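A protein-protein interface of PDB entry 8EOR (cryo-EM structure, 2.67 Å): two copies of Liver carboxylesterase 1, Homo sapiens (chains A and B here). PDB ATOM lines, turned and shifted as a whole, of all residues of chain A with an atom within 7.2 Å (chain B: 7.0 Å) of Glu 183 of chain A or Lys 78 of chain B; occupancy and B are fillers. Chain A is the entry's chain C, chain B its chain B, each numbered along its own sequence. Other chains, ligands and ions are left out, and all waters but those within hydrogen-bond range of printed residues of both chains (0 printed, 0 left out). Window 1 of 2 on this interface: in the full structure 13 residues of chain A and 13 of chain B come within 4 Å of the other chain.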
ATOM      1  N   THR A 180      14.816  13.633  24.208  1.00  0.00           N
ATOM      2  CA  THR A 180      13.936  12.543  24.607  1.00  0.00           C
ATOM      3  C   THR A 180      13.556  11.644  23.439  1.00  0.00           C
ATOM      4  O   THR A 180      12.863  10.644  23.644  1.00  0.00           O
ATOM      5  CB  THR A 180      12.666  13.095  25.262  1.00  0.00           C
ATOM      6  OG1 THR A 180      12.013  14.000  24.365  1.00  0.00           O
ATOM      7  CG2 THR A 180      12.999  13.817  26.557  1.00  0.00           C
ATOM      8  N   GLY A 181      13.999  11.971  22.227  1.00  0.00           N
ATOM      9  CA  GLY A 181      13.715  11.147  21.072  1.00  0.00           C
ATOM     10  C   GLY A 181      12.415  11.453  20.365  1.00  0.00           C
ATOM     11  O   GLY A 181      12.019  10.696  19.475  1.00  0.00           O
ATOM     12  N   ASP A 182      11.740  12.542  20.725  1.00  0.00           N
ATOM     13  CA  ASP A 182      10.451  12.874  20.135  1.00  0.00           C
ATOM     14  C   ASP A 182      10.312  14.392  20.079  1.00  0.00           C
ATOM     15  O   ASP A 182      11.284  15.130  20.256  1.00  0.00           O
ATOM     16  CB  ASP A 182       9.314  12.212  20.922  1.00  0.00           C
ATOM     17  CG  ASP A 182       9.322  12.589  22.384  1.00  0.00           C
ATOM     18  OD1 ASP A 182       9.999  13.573  22.743  1.00  0.00           O
ATOM     19  OD2 ASP A 182       8.658  11.895  23.178  1.00  0.00           O
ATOM     20  N   GLU A 183       9.084  14.855  19.829  1.00  0.00           N
ATOM     21  CA  GLU A 183       8.864  16.269  19.538  1.00  0.00           C
ATOM     22  C   GLU A 183       8.923  17.138  20.788  1.00  0.00           C
ATOM     23  O   GLU A 183       8.890  18.368  20.684  1.00  0.00           O
ATOM     24  CB  GLU A 183       7.519  16.458  18.828  1.00  0.00           C
ATOM     25  CG  GLU A 183       6.271  16.284  19.699  1.00  0.00           C
ATOM     26  CD  GLU A 183       5.990  14.840  20.058  1.00  0.00           C
ATOM     27  OE1 GLU A 183       6.784  13.962  19.670  1.00  0.00           O
ATOM     28  OE2 GLU A 183       4.971  14.580  20.731  1.00  0.00           O
ATOM     29  N   HIS A 184       9.007  16.534  21.974  1.00  0.00           N
ATOM     30  CA  HIS A 184       9.027  17.330  23.197  1.00  0.00           C
ATOM     31  C   HIS A 184      10.420  17.870  23.482  1.00  0.00           C
ATOM     32  O   HIS A 184      10.569  18.995  23.974  1.00  0.00           O
ATOM     33  CB  HIS A 184       8.510  16.499  24.366  1.00  0.00           C
ATOM     34  CG  HIS A 184       7.051  16.187  24.270  1.00  0.00           C
ATOM     35  ND1 HIS A 184       6.554  14.905  24.355  1.00  0.00           N
ATOM     36  CD2 HIS A 184       5.981  16.993  24.078  1.00  0.00           C
ATOM     37  CE1 HIS A 184       5.240  14.936  24.228  1.00  0.00           C
ATOM     38  NE2 HIS A 184       4.868  16.192  24.058  1.00  0.00           N
ATOM     39  N   SER A 185      11.454  17.079  23.200  1.00  0.00           N
ATOM     40  CA  SER A 185      12.838  17.556  23.190  1.00  0.00           C
ATOM     41  C   SER A 185      13.542  16.798  22.067  1.00  0.00           C
ATOM     42  O   SER A 185      14.057  15.697  22.276  1.00  0.00           O
ATOM     43  CB  SER A 185      13.515  17.347  24.535  1.00  0.00           C
ATOM     44  OG  SER A 185      14.729  18.073  24.617  1.00  0.00           O
ATOM     45  N   ARG A 186      13.548  17.392  20.873  1.00  0.00           N
ATOM     46  CA  ARG A 186      14.167  16.741  19.723  1.00  0.00           C
ATOM     47  C   ARG A 186      15.671  16.589  19.910  1.00  0.00           C
ATOM     48  O   ARG A 186      16.236  15.529  19.618  1.00  0.00           O
ATOM     49  CB  ARG A 186      13.870  17.536  18.455  1.00  0.00           C
ATOM     50  CG  ARG A 186      12.598  17.128  17.750  1.00  0.00           C
ATOM     51  CD  ARG A 186      12.475  17.827  16.414  1.00  0.00           C
ATOM     52  NE  ARG A 186      11.315  17.368  15.662  1.00  0.00           N
ATOM     53  CZ  ARG A 186      10.085  17.834  15.818  1.00  0.00           C
ATOM     54  NH1 ARG A 186       9.806  18.770  16.712  1.00  0.00           N
ATOM     55  NH2 ARG A 186       9.107  17.350  15.060  1.00  0.00           N
ATOM     56  N   TRP A 189      20.514  21.108  19.831  1.00  0.00           N
ATOM     57  CA  TRP A 189      20.381  22.545  20.044  1.00  0.00           C
ATOM     58  C   TRP A 189      21.662  23.278  19.668  1.00  0.00           C
ATOM     59  O   TRP A 189      21.614  24.402  19.157  1.00  0.00           O
ATOM     60  CB  TRP A 189      19.996  22.824  21.497  1.00  0.00           C
ATOM     61  CG  TRP A 189      18.857  21.973  21.981  1.00  0.00           C
ATOM     62  CD1 TRP A 189      18.849  21.163  23.077  1.00  0.00           C
ATOM     63  CD2 TRP A 189      17.566  21.838  21.375  1.00  0.00           C
ATOM     64  NE1 TRP A 189      17.636  20.537  23.194  1.00  0.00           N
ATOM     65  CE2 TRP A 189      16.829  20.933  22.162  1.00  0.00           C
ATOM     66  CE3 TRP A 189      16.959  22.393  20.244  1.00  0.00           C
ATOM     67  CZ2 TRP A 189      15.520  20.572  21.857  1.00  0.00           C
ATOM     68  CZ3 TRP A 189      15.659  22.033  19.942  1.00  0.00           C
ATOM     69  CH2 TRP A 189      14.954  21.133  20.746  1.00  0.00           C
ATOM     70  N   SER A 279       7.911  12.081  28.495  1.00  0.00           N
ATOM     71  CA  SER A 279       8.912  12.971  27.919  1.00  0.00           C
ATOM     72  C   SER A 279       8.630  14.421  28.286  1.00  0.00           C
ATOM     73  O   SER A 279       9.542  15.161  28.676  1.00  0.00           O
ATOM     74  CB  SER A 279       8.949  12.805  26.401  1.00  0.00           C
ATOM     75  OG  SER A 279       9.390  11.511  26.038  1.00  0.00           O
ATOM     76  N   ASP A 324      16.945  13.730  14.590  1.00  0.00           N
ATOM     77  CA  ASP A 324      15.769  14.336  15.194  1.00  0.00           C
ATOM     78  C   ASP A 324      14.669  14.645  14.190  1.00  0.00           C
ATOM     79  O   ASP A 324      13.535  14.910  14.603  1.00  0.00           O
ATOM     80  CB  ASP A 324      16.165  15.620  15.933  1.00  0.00           C
ATOM     81  CG  ASP A 324      16.640  16.715  14.997  1.00  0.00           C
ATOM     82  OD1 ASP A 324      17.173  16.389  13.917  1.00  0.00           O
ATOM     83  OD2 ASP A 324      16.480  17.904  15.343  1.00  0.00           O
ATOM     84  N   GLY B  31       1.016  13.817  12.485  1.00  0.00           N
ATOM     85  CA  GLY B  31       2.026  12.802  12.242  1.00  0.00           C
ATOM     86  C   GLY B  31       1.403  11.436  12.078  1.00  0.00           C
ATOM     87  O   GLY B  31       0.189  11.296  11.909  1.00  0.00           O
ATOM     88  N   LYS B  32       2.263  10.423  12.144  1.00  0.00           N
ATOM     89  CA  LYS B  32       1.835   9.043  11.961  1.00  0.00           C
ATOM     90  C   LYS B  32       1.893   8.280  13.280  1.00  0.00           C
ATOM     91  O   LYS B  32       2.758   8.522  14.124  1.00  0.00           O
ATOM     92  CB  LYS B  32       2.718   8.357  10.921  1.00  0.00           C
ATOM     93  CG  LYS B  32       2.746   9.070   9.582  1.00  0.00           C
ATOM     94  CD  LYS B  32       3.835   8.529   8.676  1.00  0.00           C
ATOM     95  CE  LYS B  32       3.595   7.076   8.312  1.00  0.00           C
ATOM     96  NZ  LYS B  32       2.276   6.874   7.648  1.00  0.00           N
ATOM     97  N   VAL B  33       0.960   7.342  13.450  1.00  0.00           N
ATOM     98  CA  VAL B  33       0.823   6.575  14.684  1.00  0.00           C
ATOM     99  C   VAL B  33       0.820   5.089  14.359  1.00  0.00           C
ATOM    100  O   VAL B  33       0.234   4.659  13.359  1.00  0.00           O
ATOM    101  CB  VAL B  33      -0.453   6.959  15.464  1.00  0.00           C
ATOM    102  CG1 VAL B  33      -0.349   8.382  15.974  1.00  0.00           C
ATOM    103  CG2 VAL B  33      -1.693   6.787  14.600  1.00  0.00           C
ATOM    104  N   LEU B  34       1.469   4.306  15.215  1.00  0.00           N
ATOM    105  CA  LEU B  34       1.604   2.866  15.042  1.00  0.00           C
ATOM    106  C   LEU B  34       0.636   2.163  15.988  1.00  0.00           C
ATOM    107  O   LEU B  34       0.712   2.345  17.207  1.00  0.00           O
ATOM    108  CB  LEU B  34       3.048   2.436  15.312  1.00  0.00           C
ATOM    109  CG  LEU B  34       3.468   0.980  15.091  1.00  0.00           C
ATOM    110  CD1 LEU B  34       3.119   0.107  16.282  1.00  0.00           C
ATOM    111  CD2 LEU B  34       2.846   0.433  13.827  1.00  0.00           C
ATOM    112  N   GLY B  35      -0.259   1.353  15.425  1.00  0.00           N
ATOM    113  CA  GLY B  35      -1.319   0.726  16.183  1.00  0.00           C
ATOM    114  C   GLY B  35      -1.044  -0.733  16.495  1.00  0.00           C
ATOM    115  O   GLY B  35       0.096  -1.198  16.527  1.00  0.00           O
ATOM    116  N   PHE B  50      -5.463   1.876  18.989  1.00  0.00           N
ATOM    117  CA  PHE B  50      -4.468   2.931  19.122  1.00  0.00           C
ATOM    118  C   PHE B  50      -4.588   3.555  20.503  1.00  0.00           C
ATOM    119  O   PHE B  50      -5.555   4.269  20.780  1.00  0.00           O
ATOM    120  CB  PHE B  50      -4.654   3.995  18.041  1.00  0.00           C
ATOM    121  CG  PHE B  50      -4.499   3.467  16.650  1.00  0.00           C
ATOM    122  CD1 PHE B  50      -5.541   2.806  16.025  1.00  0.00           C
ATOM    123  CD2 PHE B  50      -3.306   3.620  15.968  1.00  0.00           C
ATOM    124  CE1 PHE B  50      -5.396   2.313  14.746  1.00  0.00           C
ATOM    125  CE2 PHE B  50      -3.159   3.130  14.691  1.00  0.00           C
ATOM    126  CZ  PHE B  50      -4.205   2.475  14.081  1.00  0.00           C
ATOM    127  N   GLY B  52      -3.313   5.998  23.450  1.00  0.00           N
ATOM    128  CA  GLY B  52      -2.519   7.155  23.834  1.00  0.00           C
ATOM    129  C   GLY B  52      -2.179   8.098  22.702  1.00  0.00           C
ATOM    130  O   GLY B  52      -1.004   8.433  22.512  1.00  0.00           O
ATOM    131  N   ILE B  53      -3.174   8.533  21.944  1.00  0.00           N
ATOM    132  CA  ILE B  53      -2.950   9.545  20.909  1.00  0.00           C
ATOM    133  C   ILE B  53      -3.168  10.925  21.523  1.00  0.00           C
ATOM    134  O   ILE B  53      -4.254  11.187  22.058  1.00  0.00           O
ATOM    135  CB  ILE B  53      -3.880   9.322  19.723  1.00  0.00           C
ATOM    136  CG1 ILE B  53      -3.566   7.986  19.048  1.00  0.00           C
ATOM    137  CG2 ILE B  53      -3.746  10.469  18.726  1.00  0.00           C
ATOM    138  CD1 ILE B  53      -4.632   7.521  18.086  1.00  0.00           C
ATOM    139  N   PRO B  54      -2.181  11.825  21.477  1.00  0.00           N
ATOM    140  CA  PRO B  54      -2.357  13.147  22.096  1.00  0.00           C
ATOM    141  C   PRO B  54      -3.175  14.063  21.198  1.00  0.00           C
ATOM    142  O   PRO B  54      -2.825  14.281  20.037  1.00  0.00           O
ATOM    143  CB  PRO B  54      -0.920  13.651  22.253  1.00  0.00           C
ATOM    144  CG  PRO B  54      -0.199  13.028  21.116  1.00  0.00           C
ATOM    145  CD  PRO B  54      -0.834  11.677  20.895  1.00  0.00           C
ATOM    146  N   ALA B  71      -1.615  20.153  19.566  1.00  0.00           N
ATOM    147  CA  ALA B  71      -0.419  19.359  19.804  1.00  0.00           C
ATOM    148  C   ALA B  71       0.657  19.687  18.778  1.00  0.00           C
ATOM    149  O   ALA B  71       0.362  20.011  17.624  1.00  0.00           O
ATOM    150  CB  ALA B  71      -0.751  17.869  19.755  1.00  0.00           C
ATOM    151  N   GLU B  72       1.912  19.605  19.206  1.00  0.00           N
ATOM    152  CA  GLU B  72       3.022  19.838  18.296  1.00  0.00           C
ATOM    153  C   GLU B  72       3.229  18.618  17.399  1.00  0.00           C
ATOM    154  O   GLU B  72       3.218  17.484  17.883  1.00  0.00           O
ATOM    155  CB  GLU B  72       4.300  20.135  19.078  1.00  0.00           C
ATOM    156  CG  GLU B  72       4.210  21.370  19.956  1.00  0.00           C
ATOM    157  CD  GLU B  72       4.028  22.645  19.156  1.00  0.00           C
ATOM    158  OE1 GLU B  72       4.378  22.654  17.959  1.00  0.00           O
ATOM    159  OE2 GLU B  72       3.528  23.638  19.723  1.00  0.00           O
ATOM    160  N   PRO B  73       3.420  18.812  16.094  1.00  0.00           N
ATOM    161  CA  PRO B  73       3.621  17.661  15.206  1.00  0.00           C
ATOM    162  C   PRO B  73       4.919  16.925  15.502  1.00  0.00           C
ATOM    163  O   PRO B  73       5.913  17.515  15.931  1.00  0.00           O
ATOM    164  CB  PRO B  73       3.643  18.291  13.808  1.00  0.00           C
ATOM    165  CG  PRO B  73       4.029  19.702  14.032  1.00  0.00           C
ATOM    166  CD  PRO B  73       3.443  20.085  15.353  1.00  0.00           C
ATOM    167  N   TRP B  74       4.897  15.614  15.261  1.00  0.00           N
ATOM    168  CA  TRP B  74       6.052  14.750  15.465  1.00  0.00           C
ATOM    169  C   TRP B  74       6.572  14.284  14.112  1.00  0.00           C
ATOM    170  O   TRP B  74       5.841  14.312  13.117  1.00  0.00           O
ATOM    171  CB  TRP B  74       5.706  13.553  16.361  1.00  0.00           C
ATOM    172  CG  TRP B  74       4.461  12.793  15.983  1.00  0.00           C
ATOM    173  CD1 TRP B  74       4.390  11.673  15.211  1.00  0.00           C
ATOM    174  CD2 TRP B  74       3.117  13.087  16.386  1.00  0.00           C
ATOM    175  NE1 TRP B  74       3.089  11.255  15.101  1.00  0.00           N
ATOM    176  CE2 TRP B  74       2.287  12.107  15.813  1.00  0.00           C
ATOM    177  CE3 TRP B  74       2.535  14.084  17.174  1.00  0.00           C
ATOM    178  CZ2 TRP B  74       0.907  12.097  15.998  1.00  0.00           C
ATOM    179  CZ3 TRP B  74       1.167  14.073  17.357  1.00  0.00           C
ATOM    180  CH2 TRP B  74       0.368  13.085  16.771  1.00  0.00           C
ATOM    181  N   SER B  75       7.837  13.857  14.081  1.00  0.00           N
ATOM    182  CA  SER B  75       8.526  13.684  12.805  1.00  0.00           C
ATOM    183  C   SER B  75       8.473  12.240  12.318  1.00  0.00           C
ATOM    184  O   SER B  75       8.300  11.993  11.119  1.00  0.00           O
ATOM    185  CB  SER B  75       9.974  14.156  12.928  1.00  0.00           C
ATOM    186  OG  SER B  75      10.565  13.691  14.127  1.00  0.00           O
ATOM    187  N   PHE B  76       8.623  11.276  13.218  1.00  0.00           N
ATOM    188  CA  PHE B  76       8.613   9.869  12.850  1.00  0.00           C
ATOM    189  C   PHE B  76       7.404   9.180  13.471  1.00  0.00           C
ATOM    190  O   PHE B  76       6.749   9.719  14.367  1.00  0.00           O
ATOM    191  CB  PHE B  76       9.908   9.171  13.287  1.00  0.00           C
ATOM    192  CG  PHE B  76      11.155   9.869  12.822  1.00  0.00           C
ATOM    193  CD1 PHE B  76      11.488   9.902  11.479  1.00  0.00           C
ATOM    194  CD2 PHE B  76      11.994  10.492  13.729  1.00  0.00           C
ATOM    195  CE1 PHE B  76      12.632  10.546  11.051  1.00  0.00           C
ATOM    196  CE2 PHE B  76      13.138  11.136  13.305  1.00  0.00           C
ATOM    197  CZ  PHE B  76      13.456  11.162  11.966  1.00  0.00           C
ATOM    198  N   VAL B  77       7.116   7.974  12.975  1.00  0.00           N
ATOM    199  CA  VAL B  77       5.933   7.244  13.417  1.00  0.00           C
ATOM    200  C   VAL B  77       5.938   7.125  14.933  1.00  0.00           C
ATOM    201  O   VAL B  77       6.912   6.658  15.535  1.00  0.00           O
ATOM    202  CB  VAL B  77       5.880   5.862  12.751  1.00  0.00           C
ATOM    203  CG1 VAL B  77       4.648   5.102  13.209  1.00  0.00           C
ATOM    204  CG2 VAL B  77       5.892   5.998  11.237  1.00  0.00           C
ATOM    205  N   LYS B  78       4.840   7.543  15.556  1.00  0.00           N
ATOM    206  CA  LYS B  78       4.694   7.467  17.001  1.00  0.00           C
ATOM    207  C   LYS B  78       4.172   6.094  17.396  1.00  0.00           C
ATOM    208  O   LYS B  78       3.236   5.575  16.781  1.00  0.00           O
ATOM    209  CB  LYS B  78       3.746   8.549  17.517  1.00  0.00           C
ATOM    210  CG  LYS B  78       3.634   8.586  19.033  1.00  0.00           C
ATOM    211  CD  LYS B  78       2.549   9.538  19.499  1.00  0.00           C
ATOM    212  CE  LYS B  78       2.944  10.987  19.300  1.00  0.00           C
ATOM    213  NZ  LYS B  78       4.151  11.358  20.086  1.00  0.00           N
ATOM    214  N   ASN B  79       4.779   5.516  18.425  1.00  0.00           N
ATOM    215  CA  ASN B  79       4.349   4.221  18.924  1.00  0.00           C
ATOM    216  C   ASN B  79       3.156   4.400  19.854  1.00  0.00           C
ATOM    217  O   ASN B  79       3.244   5.096  20.870  1.00  0.00           O
ATOM    218  CB  ASN B  79       5.517   3.550  19.643  1.00  0.00           C
ATOM    219  CG  ASN B  79       5.250   2.107  19.984  1.00  0.00           C
ATOM    220  OD1 ASN B  79       4.199   1.557  19.660  1.00  0.00           O
ATOM    221  ND2 ASN B  79       6.214   1.478  20.640  1.00  0.00           N
ATOM    222  N   ALA B  80       2.039   3.770  19.504  1.00  0.00           N
ATOM    223  CA  ALA B  80       0.751   4.019  20.151  1.00  0.00           C
ATOM    224  C   ALA B  80       0.150   2.711  20.653  1.00  0.00           C
ATOM    225  O   ALA B  80      -1.025   2.414  20.435  1.00  0.00           O
ATOM    226  CB  ALA B  80      -0.204   4.726  19.190  1.00  0.00           C
ATOM    227  N   THR B  81       0.963   1.905  21.334  1.00  0.00           N
ATOM    228  CA  THR B  81       0.535   0.601  21.828  1.00  0.00           C
ATOM    229  C   THR B  81       0.603   0.500  23.347  1.00  0.00           C
ATOM    230  O   THR B  81       0.592  -0.613  23.883  1.00  0.00           O
ATOM    231  CB  THR B  81       1.384  -0.512  21.202  1.00  0.00           C
ATOM    232  OG1 THR B  81       2.740  -0.395  21.648  1.00  0.00           O
ATOM    233  CG2 THR B  81       1.346  -0.429  19.683  1.00  0.00           C
ATOM    234  N   TYR B 118      -5.029  12.594  26.321  1.00  0.00           N
ATOM    235  CA  TYR B 118      -4.882  11.559  25.308  1.00  0.00           C
ATOM    236  C   TYR B 118      -6.237  10.920  25.046  1.00  0.00           C
ATOM    237  O   TYR B 118      -7.206  11.148  25.771  1.00  0.00           O
ATOM    238  CB  TYR B 118      -3.884  10.474  25.736  1.00  0.00           C
ATOM    239  CG  TYR B 118      -2.501  10.987  26.052  1.00  0.00           C
ATOM    240  CD1 TYR B 118      -1.563  11.166  25.049  1.00  0.00           C
ATOM    241  CD2 TYR B 118      -2.133  11.285  27.356  1.00  0.00           C
ATOM    242  CE1 TYR B 118      -0.301  11.632  25.331  1.00  0.00           C
ATOM    243  CE2 TYR B 118      -0.873  11.750  27.648  1.00  0.00           C
ATOM    244  CZ  TYR B 118       0.040  11.923  26.630  1.00  0.00           C
ATOM    245  OH  TYR B 118       1.302  12.388  26.914  1.00  0.00           O
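O of Lys 32 of chain B sits at hydrogen-bond distance from NE1 of Trp 74 of chain B.
The backbone NH (N) of Lys 78 of chain B lies within hydrogen-bond range of the backbone carbonyl oxygen (O) of Lys 32 of chain B, at 2.7 Å.
The backbone NH (N) of Leu 34 of chain B is in hydrogen-bond range of the backbone carbonyl oxygen (O) of Lys 78 of chain B, at 2.7 Å.
The guanidinium group (NE) of Arg 186 of chain A lies within hydrogen-bond range of the backbone carbonyl oxygen (O) of Asp 324 of chain A, 3.5 Å away.
Of the printed residues of chain B, Glu 183 of chain A touches Glu 72 (3.7 Å), Pro 73 (3.5 Å), Trp 74 (3.5 Å) and Lys 78 (3.4 Å).
Printed residues of chain B within 4 Å of Arg 186 of chain A: Pro 73 and Ser 75.
Ser 279 of chain A touches none of the printed residues of chain B.
Of the printed residues of chain B, Asp 324 of chain A touches Ser 75 and Phe 76.
Of the printed residues of chain A, Glu 72 of chain B touches Glu 183 (3.7 Å).
Of the printed residues of chain A, Trp 74 of chain B touches Glu 183.
Printed residues of chain A within 4 Å of Ser 75 of chain B: Arg 186 and Asp 324.
Of chain A, only Glu 183 (3.4 Å) comes within 4 Å of Lys 78 of chain B.
The nearest residue of chain A that does not touch Lys 78 of chain B is Asp 182 of chain A (5.3 Å).
O of Pro 73 of chain B is in hydrogen-bond range of NH2 of Arg 186 of chain A, 3.3 Å away.
O of Asp 324 of chain A sits at hydrogen-bond distance from OG of Ser 75 of chain B.
The side-chain amino group (NZ) of Lys 78 of chain B lies within salt-bridge range of the side-chain carboxylate (OE2) of Glu 183 of chain A (3.4 Å).
Among the printed residues, merely in contact across the chains: Glu 183 of chain A with Pro 73 of chain B, Glu 183 of chain A with Trp 74 of chain B, Glu 183 of chain A with Glu 72 of chain B, Arg 186 of chain A with Ser 75 of chain B and Asp 324 of chain A with Phe 76 of chain B.
No position is printed for both chains.
Of the 21 printed residues of chain B, 6 touch a printed residue of chain A.
Of the 10 printed residues of chain A, 3 touch a printed residue of chain B.
Printed residues of chain A that touch a printed residue of chain B: Glu 183, Arg 186 and Asp 324.
Among the printed residues, 8 pairs touch across the chains.
Among the printed residues, Asp or Glu carboxylates within 4 Å of a Lys or Arg side-chain nitrogen of the other chain: Glu 183 of chain A with Lys 78 of chain B.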
